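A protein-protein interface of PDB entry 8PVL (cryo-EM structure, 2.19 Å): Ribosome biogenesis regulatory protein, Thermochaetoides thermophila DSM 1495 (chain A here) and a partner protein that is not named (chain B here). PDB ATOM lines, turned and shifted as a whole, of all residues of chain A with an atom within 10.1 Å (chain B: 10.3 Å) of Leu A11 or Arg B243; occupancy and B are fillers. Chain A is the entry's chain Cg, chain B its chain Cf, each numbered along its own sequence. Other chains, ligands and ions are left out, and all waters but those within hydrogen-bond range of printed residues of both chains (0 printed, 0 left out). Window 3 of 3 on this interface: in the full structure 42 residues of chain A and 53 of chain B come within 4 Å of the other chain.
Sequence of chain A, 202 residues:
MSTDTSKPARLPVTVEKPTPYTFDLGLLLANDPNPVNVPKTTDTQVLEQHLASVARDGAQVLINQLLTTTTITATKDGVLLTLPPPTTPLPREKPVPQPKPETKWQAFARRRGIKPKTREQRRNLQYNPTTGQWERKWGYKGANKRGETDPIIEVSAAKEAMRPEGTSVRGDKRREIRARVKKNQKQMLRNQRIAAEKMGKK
The guanidinium group (NH1) of Arg A56 sits close to the guanidinium group (NH1) of Arg B243 (3.3 Å).
The backbone carbonyl oxygen (O) of Pro B242 lies within hydrogen-bond range of the side-chain amide nitrogen (NE2) of Gln A60 (3.2 Å).
The guanidinium group (NH1) of Arg B243 lies within hydrogen-bond range of the backbone carbonyl oxygen (O) of Pro A12, 2.7 Å away.
N of Val B244 sits at hydrogen-bond distance from OE1 of Gln A60 (3.1 Å).
The side-chain hydroxyl (OG) of Ser B237 sits at hydrogen-bond distance from the backbone carbonyl oxygen (O) of Leu B241 (2.8 Å).
OD1 of Asn A64 lies within hydrogen-bond range of NE2 of Gln A60 (2.9 Å).
The side-chain amide nitrogen of Gln A60 is in hydrogen-bond range of the backbone carbonyl oxygen of Val A13, 3.1 Å away.
The guanidinium group of Arg B243 is in salt-bridge range of the side-chain carboxylate of Glu B245 (3.2 Å).
O of Leu B241 is in hydrogen-bond range of OG1 of Thr B239, 3.1 Å away.
N of Lys B235 is in hydrogen-bond range of O of Arg B243 (2.9 Å).
Among the printed residues, pairs that only touch across the chains: Leu A11 with Arg B243, Val A13 with Ser B237, Val A13 with Thr B239, Val A13 with Leu B241, Val A13 with Pro B242, Ala A52 with Val B246, Arg A56 with Val B244, Arg A56 with Val B246, Ala A59 with Val B244, Gln A60 with Arg B243, Asn A64 with Leu B241 and Leu A67 with Pro B242.
Pro A12 touches just one residue of chain B: Arg B243 (2.7 Å).
Glu A16 touches none of the printed residues of chain B.
Of the printed residues of chain B, Ala A52 touches Val B246.
Of the printed residues of chain B, Ala A59 touches Val B244 (3.8 Å).
Ile A63 touches none of the printed residues of chain B.
No residue of chain A comes within 4 Å of Lys B235.
Of the printed residues of chain A, Ser B237 touches Val A13 (3.3 Å).
Of the printed residues of chain A, Pro B242 touches Val A13, Gln A60 and Leu A67.
Of the printed residues of chain A, Val B244 touches Arg A56, Ala A59 and Gln A60.
The nearest printed residue of chain A that does not touch Arg B243 is Val A13 (4.01 Å).
The nearest printed residue of chain B that does not touch Ala A59 is Ile B232 (4.2 Å).
Hydrophobic or aromatic side chains of chain B within 4 Å of the printed part of chain A: Leu B241, Pro B242, Val B244 and Val B246.
Of the 18 printed residues of chain A, 9 touch a printed residue of chain B.
Hydrophobic or aromatic side chains of chain A within 4 Å of the printed part of chain B: Leu A11, Pro A12, Val A13, Ala A59 and Leu A67.
Among the printed residues, 16 pairs touch across the chains.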
ATOM      1  N   LEU A  11      18.621  33.706  -1.084  1.00  0.00           N
ATOM      2  CA  LEU A  11      19.408  33.001  -2.088  1.00  0.00           C
ATOM      3  C   LEU A  11      18.688  31.740  -2.556  1.00  0.00           C
ATOM      4  O   LEU A  11      18.155  30.988  -1.741  1.00  0.00           O
ATOM      5  CB  LEU A  11      20.791  32.652  -1.538  1.00  0.00           C
ATOM      6  CG  LEU A  11      21.756  33.828  -1.378  1.00  0.00           C
ATOM      7  CD1 LEU A  11      23.069  33.371  -0.766  1.00  0.00           C
ATOM      8  CD2 LEU A  11      21.995  34.504  -2.719  1.00  0.00           C
ATOM      9  N   PRO A  12      18.666  31.515  -3.868  1.00  0.00           N
ATOM     10  CA  PRO A  12      17.949  30.356  -4.406  1.00  0.00           C
ATOM     11  C   PRO A  12      18.665  29.048  -4.110  1.00  0.00           C
ATOM     12  O   PRO A  12      19.881  29.004  -3.910  1.00  0.00           O
ATOM     13  CB  PRO A  12      17.910  30.634  -5.912  1.00  0.00           C
ATOM     14  CG  PRO A  12      19.120  31.466  -6.157  1.00  0.00           C
ATOM     15  CD  PRO A  12      19.282  32.325  -4.934  1.00  0.00           C
ATOM     16  N   VAL A  13      17.883  27.970  -4.085  1.00  0.00           N
ATOM     17  CA  VAL A  13      18.398  26.619  -3.904  1.00  0.00           C
ATOM     18  C   VAL A  13      18.222  25.778  -5.159  1.00  0.00           C
ATOM     19  O   VAL A  13      18.450  24.566  -5.125  1.00  0.00           O
ATOM     20  CB  VAL A  13      17.749  25.929  -2.695  1.00  0.00           C
ATOM     21  CG1 VAL A  13      18.190  26.601  -1.411  1.00  0.00           C
ATOM     22  CG2 VAL A  13      16.235  25.950  -2.822  1.00  0.00           C
ATOM     23  N   THR A  14      17.816  26.392  -6.266  1.00  0.00           N
ATOM     24  CA  THR A  14      17.624  25.695  -7.529  1.00  0.00           C
ATOM     25  C   THR A  14      18.421  26.409  -8.607  1.00  0.00           C
ATOM     26  O   THR A  14      18.357  27.638  -8.715  1.00  0.00           O
ATOM     27  CB  THR A  14      16.142  25.645  -7.917  1.00  0.00           C
ATOM     28  OG1 THR A  14      15.358  25.279  -6.775  1.00  0.00           O
ATOM     29  CG2 THR A  14      15.915  24.631  -9.027  1.00  0.00           C
ATOM     30  N   VAL A  15      19.171  25.649  -9.395  1.00  0.00           N
ATOM     31  CA  VAL A  15      19.909  26.205 -10.522  1.00  0.00           C
ATOM     32  C   VAL A  15      19.144  25.874 -11.795  1.00  0.00           C
ATOM     33  O   VAL A  15      18.394  24.891 -11.863  1.00  0.00           O
ATOM     34  CB  VAL A  15      21.373  25.701 -10.574  1.00  0.00           C
ATOM     35  CG1 VAL A  15      21.876  25.379  -9.172  1.00  0.00           C
ATOM     36  CG2 VAL A  15      21.539  24.503 -11.503  1.00  0.00           C
ATOM     37  N   GLU A  16      19.294  26.739 -12.796  1.00  0.00           N
ATOM     38  CA  GLU A  16      18.612  26.594 -14.075  1.00  0.00           C
ATOM     39  C   GLU A  16      19.654  26.594 -15.181  1.00  0.00           C
ATOM     40  O   GLU A  16      20.436  27.542 -15.303  1.00  0.00           O
ATOM     41  CB  GLU A  16      17.594  27.718 -14.292  1.00  0.00           C
ATOM     42  CG  GLU A  16      16.757  28.076 -13.064  1.00  0.00           C
ATOM     43  CD  GLU A  16      15.608  27.112 -12.804  1.00  0.00           C
ATOM     44  OE1 GLU A  16      15.448  26.132 -13.563  1.00  0.00           O
ATOM     45  OE2 GLU A  16      14.860  27.336 -11.830  1.00  0.00           O
ATOM     46  N   ALA A  52      34.516  28.049  -9.155  1.00  0.00           N
ATOM     47  CA  ALA A  52      33.815  27.844  -7.896  1.00  0.00           C
ATOM     48  C   ALA A  52      32.308  27.987  -8.058  1.00  0.00           C
ATOM     49  O   ALA A  52      31.555  27.298  -7.369  1.00  0.00           O
ATOM     50  CB  ALA A  52      34.333  28.818  -6.839  1.00  0.00           C
ATOM     51  N   SER A  53      31.847  28.858  -8.961  1.00  0.00           N
ATOM     52  CA  SER A  53      30.417  28.943  -9.236  1.00  0.00           C
ATOM     53  C   SER A  53      29.902  27.666  -9.888  1.00  0.00           C
ATOM     54  O   SER A  53      28.821  27.177  -9.534  1.00  0.00           O
ATOM     55  CB  SER A  53      30.125  30.151 -10.124  1.00  0.00           C
ATOM     56  OG  SER A  53      30.878  30.091 -11.320  1.00  0.00           O
ATOM     57  N   ALA A  55      31.216  24.674  -9.555  1.00  0.00           N
ATOM     58  CA  ALA A  55      31.222  23.698  -8.469  1.00  0.00           C
ATOM     59  C   ALA A  55      30.053  23.912  -7.517  1.00  0.00           C
ATOM     60  O   ALA A  55      29.497  22.948  -6.981  1.00  0.00           O
ATOM     61  CB  ALA A  55      32.538  23.784  -7.708  1.00  0.00           C
ATOM     62  N   ARG A  56      29.684  25.173  -7.285  1.00  0.00           N
ATOM     63  CA  ARG A  56      28.558  25.493  -6.418  1.00  0.00           C
ATOM     64  C   ARG A  56      27.253  24.949  -6.981  1.00  0.00           C
ATOM     65  O   ARG A  56      26.468  24.335  -6.249  1.00  0.00           O
ATOM     66  CB  ARG A  56      28.481  27.009  -6.235  1.00  0.00           C
ATOM     67  CG  ARG A  56      28.128  27.479  -4.842  1.00  0.00           C
ATOM     68  CD  ARG A  56      26.643  27.373  -4.597  1.00  0.00           C
ATOM     69  NE  ARG A  56      25.858  27.751  -5.765  1.00  0.00           N
ATOM     70  CZ  ARG A  56      24.548  27.581  -5.867  1.00  0.00           C
ATOM     71  NH1 ARG A  56      23.842  27.050  -4.882  1.00  0.00           N
ATOM     72  NH2 ARG A  56      23.931  27.950  -6.985  1.00  0.00           N
ATOM     73  N   ASP A  57      27.013  25.152  -8.283  1.00  0.00           N
ATOM     74  CA  ASP A  57      25.800  24.603  -8.894  1.00  0.00           C
ATOM     75  C   ASP A  57      25.797  23.079  -8.862  1.00  0.00           C
ATOM     76  O   ASP A  57      24.760  22.463  -8.579  1.00  0.00           O
ATOM     77  CB  ASP A  57      25.620  25.092 -10.333  1.00  0.00           C
ATOM     78  CG  ASP A  57      26.084  26.510 -10.540  1.00  0.00           C
ATOM     79  OD1 ASP A  57      25.712  27.385  -9.730  1.00  0.00           O
ATOM     80  OD2 ASP A  57      26.807  26.760 -11.528  1.00  0.00           O
ATOM     81  N   GLY A  58      26.949  22.456  -9.144  1.00  0.00           N
ATOM     82  CA  GLY A  58      27.012  21.000  -9.113  1.00  0.00           C
ATOM     83  C   GLY A  58      26.754  20.421  -7.733  1.00  0.00           C
ATOM     84  O   GLY A  58      25.979  19.469  -7.580  1.00  0.00           O
ATOM     85  N   ALA A  59      27.377  21.005  -6.705  1.00  0.00           N
ATOM     86  CA  ALA A  59      27.159  20.547  -5.338  1.00  0.00           C
ATOM     87  C   ALA A  59      25.723  20.784  -4.897  1.00  0.00           C
ATOM     88  O   ALA A  59      25.135  19.944  -4.205  1.00  0.00           O
ATOM     89  CB  ALA A  59      28.134  21.241  -4.389  1.00  0.00           C
ATOM     90  N   GLN A  60      25.135  21.918  -5.297  1.00  0.00           N
ATOM     91  CA  GLN A  60      23.760  22.221  -4.917  1.00  0.00           C
ATOM     92  C   GLN A  60      22.782  21.225  -5.526  1.00  0.00           C
ATOM     93  O   GLN A  60      21.886  20.723  -4.836  1.00  0.00           O
ATOM     94  CB  GLN A  60      23.407  23.648  -5.337  1.00  0.00           C
ATOM     95  CG  GLN A  60      21.940  24.005  -5.161  1.00  0.00           C
ATOM     96  CD  GLN A  60      21.588  24.353  -3.729  1.00  0.00           C
ATOM     97  OE1 GLN A  60      22.155  25.274  -3.145  1.00  0.00           O
ATOM     98  NE2 GLN A  60      20.643  23.618  -3.158  1.00  0.00           N
ATOM     99  N   VAL A  61      22.944  20.908  -6.816  1.00  0.00           N
ATOM    100  CA  VAL A  61      22.003  19.971  -7.427  1.00  0.00           C
ATOM    101  C   VAL A  61      22.227  18.555  -6.904  1.00  0.00           C
ATOM    102  O   VAL A  61      21.263  17.788  -6.763  1.00  0.00           O
ATOM    103  CB  VAL A  61      22.049  20.034  -8.968  1.00  0.00           C
ATOM    104  CG1 VAL A  61      21.665  21.421  -9.445  1.00  0.00           C
ATOM    105  CG2 VAL A  61      23.401  19.629  -9.521  1.00  0.00           C
ATOM    106  N   ILE A  63      23.166  17.833  -3.778  1.00  0.00           N
ATOM    107  CA  ILE A  63      22.551  17.828  -2.454  1.00  0.00           C
ATOM    108  C   ILE A  63      21.031  17.773  -2.567  1.00  0.00           C
ATOM    109  O   ILE A  63      20.370  17.038  -1.824  1.00  0.00           O
ATOM    110  CB  ILE A  63      23.031  19.047  -1.642  1.00  0.00           C
ATOM    111  CG1 ILE A  63      24.486  18.857  -1.210  1.00  0.00           C
ATOM    112  CG2 ILE A  63      22.161  19.282  -0.416  1.00  0.00           C
ATOM    113  CD1 ILE A  63      24.723  17.619  -0.378  1.00  0.00           C
ATOM    114  N   ASN A  64      20.458  18.526  -3.516  1.00  0.00           N
ATOM    115  CA  ASN A  64      19.011  18.497  -3.720  1.00  0.00           C
ATOM    116  C   ASN A  64      18.530  17.115  -4.146  1.00  0.00           C
ATOM    117  O   ASN A  64      17.530  16.609  -3.619  1.00  0.00           O
ATOM    118  CB  ASN A  64      18.606  19.542  -4.761  1.00  0.00           C
ATOM    119  CG  ASN A  64      18.851  20.960  -4.292  1.00  0.00           C
ATOM    120  OD1 ASN A  64      19.043  21.209  -3.104  1.00  0.00           O
ATOM    121  ND2 ASN A  64      18.848  21.901  -5.228  1.00  0.00           N
ATOM    122  N   LEU A  67      18.813  14.674  -1.161  1.00  0.00           N
ATOM    123  CA  LEU A  67      17.849  14.931  -0.101  1.00  0.00           C
ATOM    124  C   LEU A  67      16.405  14.746  -0.548  1.00  0.00           C
ATOM    125  O   LEU A  67      15.520  14.650   0.309  1.00  0.00           O
ATOM    126  CB  LEU A  67      18.034  16.346   0.448  1.00  0.00           C
ATOM    127  CG  LEU A  67      19.287  16.574   1.294  1.00  0.00           C
ATOM    128  CD1 LEU A  67      19.319  17.990   1.838  1.00  0.00           C
ATOM    129  CD2 LEU A  67      19.369  15.562   2.420  1.00  0.00           C
ATOM    130  N   GLY B 231      35.292  22.163  -0.179  1.00  0.00           N
ATOM    131  CA  GLY B 231      34.501  21.834   0.987  1.00  0.00           C
ATOM    132  C   GLY B 231      33.136  22.493   0.907  1.00  0.00           C
ATOM    133  O   GLY B 231      32.981  23.562   0.331  1.00  0.00           O
ATOM    134  N   ILE B 232      32.141  21.848   1.506  1.00  0.00           N
ATOM    135  CA  ILE B 232      30.742  22.216   1.320  1.00  0.00           C
ATOM    136  C   ILE B 232      30.180  22.731   2.637  1.00  0.00           C
ATOM    137  O   ILE B 232      30.273  22.055   3.668  1.00  0.00           O
ATOM    138  CB  ILE B 232      29.924  21.025   0.794  1.00  0.00           C
ATOM    139  CG1 ILE B 232      30.300  20.735  -0.657  1.00  0.00           C
ATOM    140  CG2 ILE B 232      28.435  21.294   0.907  1.00  0.00           C
ATOM    141  CD1 ILE B 232      29.895  19.366  -1.117  1.00  0.00           C
ATOM    142  N   ARG B 233      29.603  23.930   2.599  1.00  0.00           N
ATOM    143  CA  ARG B 233      28.911  24.524   3.732  1.00  0.00           C
ATOM    144  C   ARG B 233      27.449  24.735   3.368  1.00  0.00           C
ATOM    145  O   ARG B 233      27.132  25.131   2.243  1.00  0.00           O
ATOM    146  CB  ARG B 233      29.545  25.857   4.133  1.00  0.00           C
ATOM    147  CG  ARG B 233      30.933  25.728   4.741  1.00  0.00           C
ATOM    148  CD  ARG B 233      31.562  27.084   5.059  1.00  0.00           C
ATOM    149  NE  ARG B 233      30.786  28.214   4.559  1.00  0.00           N
ATOM    150  CZ  ARG B 233      31.053  28.875   3.441  1.00  0.00           C
ATOM    151  NH1 ARG B 233      32.074  28.543   2.669  1.00  0.00           N
ATOM    152  NH2 ARG B 233      30.276  29.896   3.088  1.00  0.00           N
ATOM    153  N   THR B 234      26.558  24.469   4.319  1.00  0.00           N
ATOM    154  CA  THR B 234      25.126  24.608   4.111  1.00  0.00           C
ATOM    155  C   THR B 234      24.578  25.716   5.000  1.00  0.00           C
ATOM    156  O   THR B 234      24.959  25.832   6.169  1.00  0.00           O
ATOM    157  CB  THR B 234      24.389  23.298   4.402  1.00  0.00           C
ATOM    158  OG1 THR B 234      24.625  22.906   5.759  1.00  0.00           O
ATOM    159  CG2 THR B 234      24.876  22.200   3.471  1.00  0.00           C
ATOM    160  N   LYS B 235      23.683  26.526   4.440  1.00  0.00           N
ATOM    161  CA  LYS B 235      23.047  27.617   5.158  1.00  0.00           C
ATOM    162  C   LYS B 235      21.534  27.508   5.033  1.00  0.00           C
ATOM    163  O   LYS B 235      21.009  26.893   4.101  1.00  0.00           O
ATOM    164  CB  LYS B 235      23.504  28.983   4.632  1.00  0.00           C
ATOM    165  CG  LYS B 235      24.942  29.340   4.970  1.00  0.00           C
ATOM    166  CD  LYS B 235      25.180  30.848   4.938  1.00  0.00           C
ATOM    167  CE  LYS B 235      24.567  31.512   3.711  1.00  0.00           C
ATOM    168  NZ  LYS B 235      25.083  30.952   2.434  1.00  0.00           N
ATOM    169  N   ARG B 236      20.837  28.108   5.994  1.00  0.00           N
ATOM    170  CA  ARG B 236      19.385  28.173   5.933  1.00  0.00           C
ATOM    171  C   ARG B 236      18.946  29.100   4.807  1.00  0.00           C
ATOM    172  O   ARG B 236      19.514  30.178   4.609  1.00  0.00           O
ATOM    173  CB  ARG B 236      18.814  28.656   7.265  1.00  0.00           C
ATOM    174  CG  ARG B 236      19.230  27.815   8.456  1.00  0.00           C
ATOM    175  CD  ARG B 236      18.559  28.282   9.733  1.00  0.00           C
ATOM    176  NE  ARG B 236      18.943  27.463  10.876  1.00  0.00           N
ATOM    177  CZ  ARG B 236      18.357  26.322  11.211  1.00  0.00           C
ATOM    178  NH1 ARG B 236      17.344  25.836  10.513  1.00  0.00           N
ATOM    179  NH2 ARG B 236      18.798  25.653  12.271  1.00  0.00           N
ATOM    180  N   SER B 237      17.929  28.672   4.063  1.00  0.00           N
ATOM    181  CA  SER B 237      17.436  29.424   2.921  1.00  0.00           C
ATOM    182  C   SER B 237      15.949  29.732   2.998  1.00  0.00           C
ATOM    183  O   SER B 237      15.405  30.316   2.053  1.00  0.00           O
ATOM    184  CB  SER B 237      17.728  28.661   1.623  1.00  0.00           C
ATOM    185  OG  SER B 237      16.990  27.452   1.577  1.00  0.00           O
ATOM    186  N   GLY B 238      15.278  29.361   4.084  1.00  0.00           N
ATOM    187  CA  GLY B 238      13.852  29.562   4.207  1.00  0.00           C
ATOM    188  C   GLY B 238      13.001  28.447   3.647  1.00  0.00           C
ATOM    189  O   GLY B 238      11.778  28.468   3.841  1.00  0.00           O
ATOM    190  N   THR B 239      13.599  27.478   2.963  1.00  0.00           N
ATOM    191  CA  THR B 239      12.906  26.309   2.438  1.00  0.00           C
ATOM    192  C   THR B 239      13.452  25.056   3.114  1.00  0.00           C
ATOM    193  O   THR B 239      14.290  25.124   4.017  1.00  0.00           O
ATOM    194  CB  THR B 239      13.053  26.209   0.916  1.00  0.00           C
ATOM    195  OG1 THR B 239      14.342  25.672   0.593  1.00  0.00           O
ATOM    196  CG2 THR B 239      12.900  27.576   0.262  1.00  0.00           C
ATOM    197  N   ARG B 240      12.958  23.899   2.670  1.00  0.00           N
ATOM    198  CA  ARG B 240      13.460  22.634   3.195  1.00  0.00           C
ATOM    199  C   ARG B 240      14.887  22.370   2.731  1.00  0.00           C
ATOM    200  O   ARG B 240      15.731  21.932   3.522  1.00  0.00           O
ATOM    201  CB  ARG B 240      12.538  21.490   2.773  1.00  0.00           C
ATOM    202  CG  ARG B 240      11.240  21.418   3.557  1.00  0.00           C
ATOM    203  CD  ARG B 240      11.498  21.148   5.030  1.00  0.00           C
ATOM    204  NE  ARG B 240      11.976  19.790   5.261  1.00  0.00           N
ATOM    205  CZ  ARG B 240      12.617  19.398   6.353  1.00  0.00           C
ATOM    206  NH1 ARG B 240      12.877  20.238   7.342  1.00  0.00           N
ATOM    207  NH2 ARG B 240      13.008  18.130   6.457  1.00  0.00           N
ATOM    208  N   LEU B 241      15.174  22.626   1.460  1.00  0.00           N
ATOM    209  CA  LEU B 241      16.510  22.389   0.936  1.00  0.00           C
ATOM    210  C   LEU B 241      17.468  23.478   1.417  1.00  0.00           C
ATOM    211  O   LEU B 241      17.113  24.660   1.424  1.00  0.00           O
ATOM    212  CB  LEU B 241      16.488  22.348  -0.589  1.00  0.00           C
ATOM    213  CG  LEU B 241      15.574  21.294  -1.217  1.00  0.00           C
ATOM    214  CD1 LEU B 241      15.637  21.358  -2.733  1.00  0.00           C
ATOM    215  CD2 LEU B 241      15.941  19.907  -0.721  1.00  0.00           C
ATOM    216  N   PRO B 242      18.678  23.115   1.828  1.00  0.00           N
ATOM    217  CA  PRO B 242      19.646  24.121   2.268  1.00  0.00           C
ATOM    218  C   PRO B 242      20.332  24.802   1.092  1.00  0.00           C
ATOM    219  O   PRO B 242      20.292  24.340  -0.048  1.00  0.00           O
ATOM    220  CB  PRO B 242      20.648  23.306   3.087  1.00  0.00           C
ATOM    221  CG  PRO B 242      20.616  21.961   2.451  1.00  0.00           C
ATOM    222  CD  PRO B 242      19.199  21.746   1.983  1.00  0.00           C
ATOM    223  N   ARG B 243      20.973  25.925   1.400  1.00  0.00           N
ATOM    224  CA  ARG B 243      21.751  26.680   0.427  1.00  0.00           C
ATOM    225  C   ARG B 243      23.212  26.262   0.542  1.00  0.00           C
ATOM    226  O   ARG B 243      23.838  26.451   1.590  1.00  0.00           O
ATOM    227  CB  ARG B 243      21.590  28.183   0.652  1.00  0.00           C
ATOM    228  CG  ARG B 243      22.627  29.046  -0.049  1.00  0.00           C
ATOM    229  CD  ARG B 243      22.337  29.184  -1.532  1.00  0.00           C
ATOM    230  NE  ARG B 243      23.334  30.013  -2.198  1.00  0.00           N
ATOM    231  CZ  ARG B 243      23.309  30.329  -3.485  1.00  0.00           C
ATOM    232  NH1 ARG B 243      22.348  29.897  -4.284  1.00  0.00           N
ATOM    233  NH2 ARG B 243      24.273  31.097  -3.983  1.00  0.00           N
ATOM    234  N   VAL B 244      23.747  25.695  -0.532  1.00  0.00           N
ATOM    235  CA  VAL B 244      25.105  25.166  -0.541  1.00  0.00           C
ATOM    236  C   VAL B 244      26.083  26.306  -0.794  1.00  0.00           C
ATOM    237  O   VAL B 244      25.790  27.234  -1.554  1.00  0.00           O
ATOM    238  CB  VAL B 244      25.225  24.054  -1.604  1.00  0.00           C
ATOM    239  CG1 VAL B 244      26.654  23.549  -1.750  1.00  0.00           C
ATOM    240  CG2 VAL B 244      24.293  22.904  -1.263  1.00  0.00           C
ATOM    241  N   GLU B 245      27.226  26.275  -0.108  1.00  0.00           N
ATOM    242  CA  GLU B 245      28.353  27.145  -0.411  1.00  0.00           C
ATOM    243  C   GLU B 245      29.625  26.312  -0.453  1.00  0.00           C
ATOM    244  O   GLU B 245      29.745  25.303   0.245  1.00  0.00           O
ATOM    245  CB  GLU B 245      28.497  28.276   0.613  1.00  0.00           C
ATOM    246  CG  GLU B 245      27.355  29.275   0.603  1.00  0.00           C
ATOM    247  CD  GLU B 245      27.332  30.136  -0.649  1.00  0.00           C
ATOM    248  OE1 GLU B 245      28.402  30.332  -1.264  1.00  0.00           O
ATOM    249  OE2 GLU B 245      26.241  30.615  -1.020  1.00  0.00           O
ATOM    250  N   VAL B 246      30.577  26.739  -1.279  1.00  0.00           N
ATOM    251  CA  VAL B 246      31.808  25.986  -1.481  1.00  0.00           C
ATOM    252  C   VAL B 246      33.005  26.844  -1.099  1.00  0.00           C
ATOM    253  O   VAL B 246      32.979  28.074  -1.201  1.00  0.00           O
ATOM    254  CB  VAL B 246      31.946  25.474  -2.932  1.00  0.00           C
ATOM    255  CG1 VAL B 246      30.921  24.390  -3.211  1.00  0.00           C
ATOM    256  CG2 VAL B 246      31.800  26.617  -3.919  1.00  0.00           C
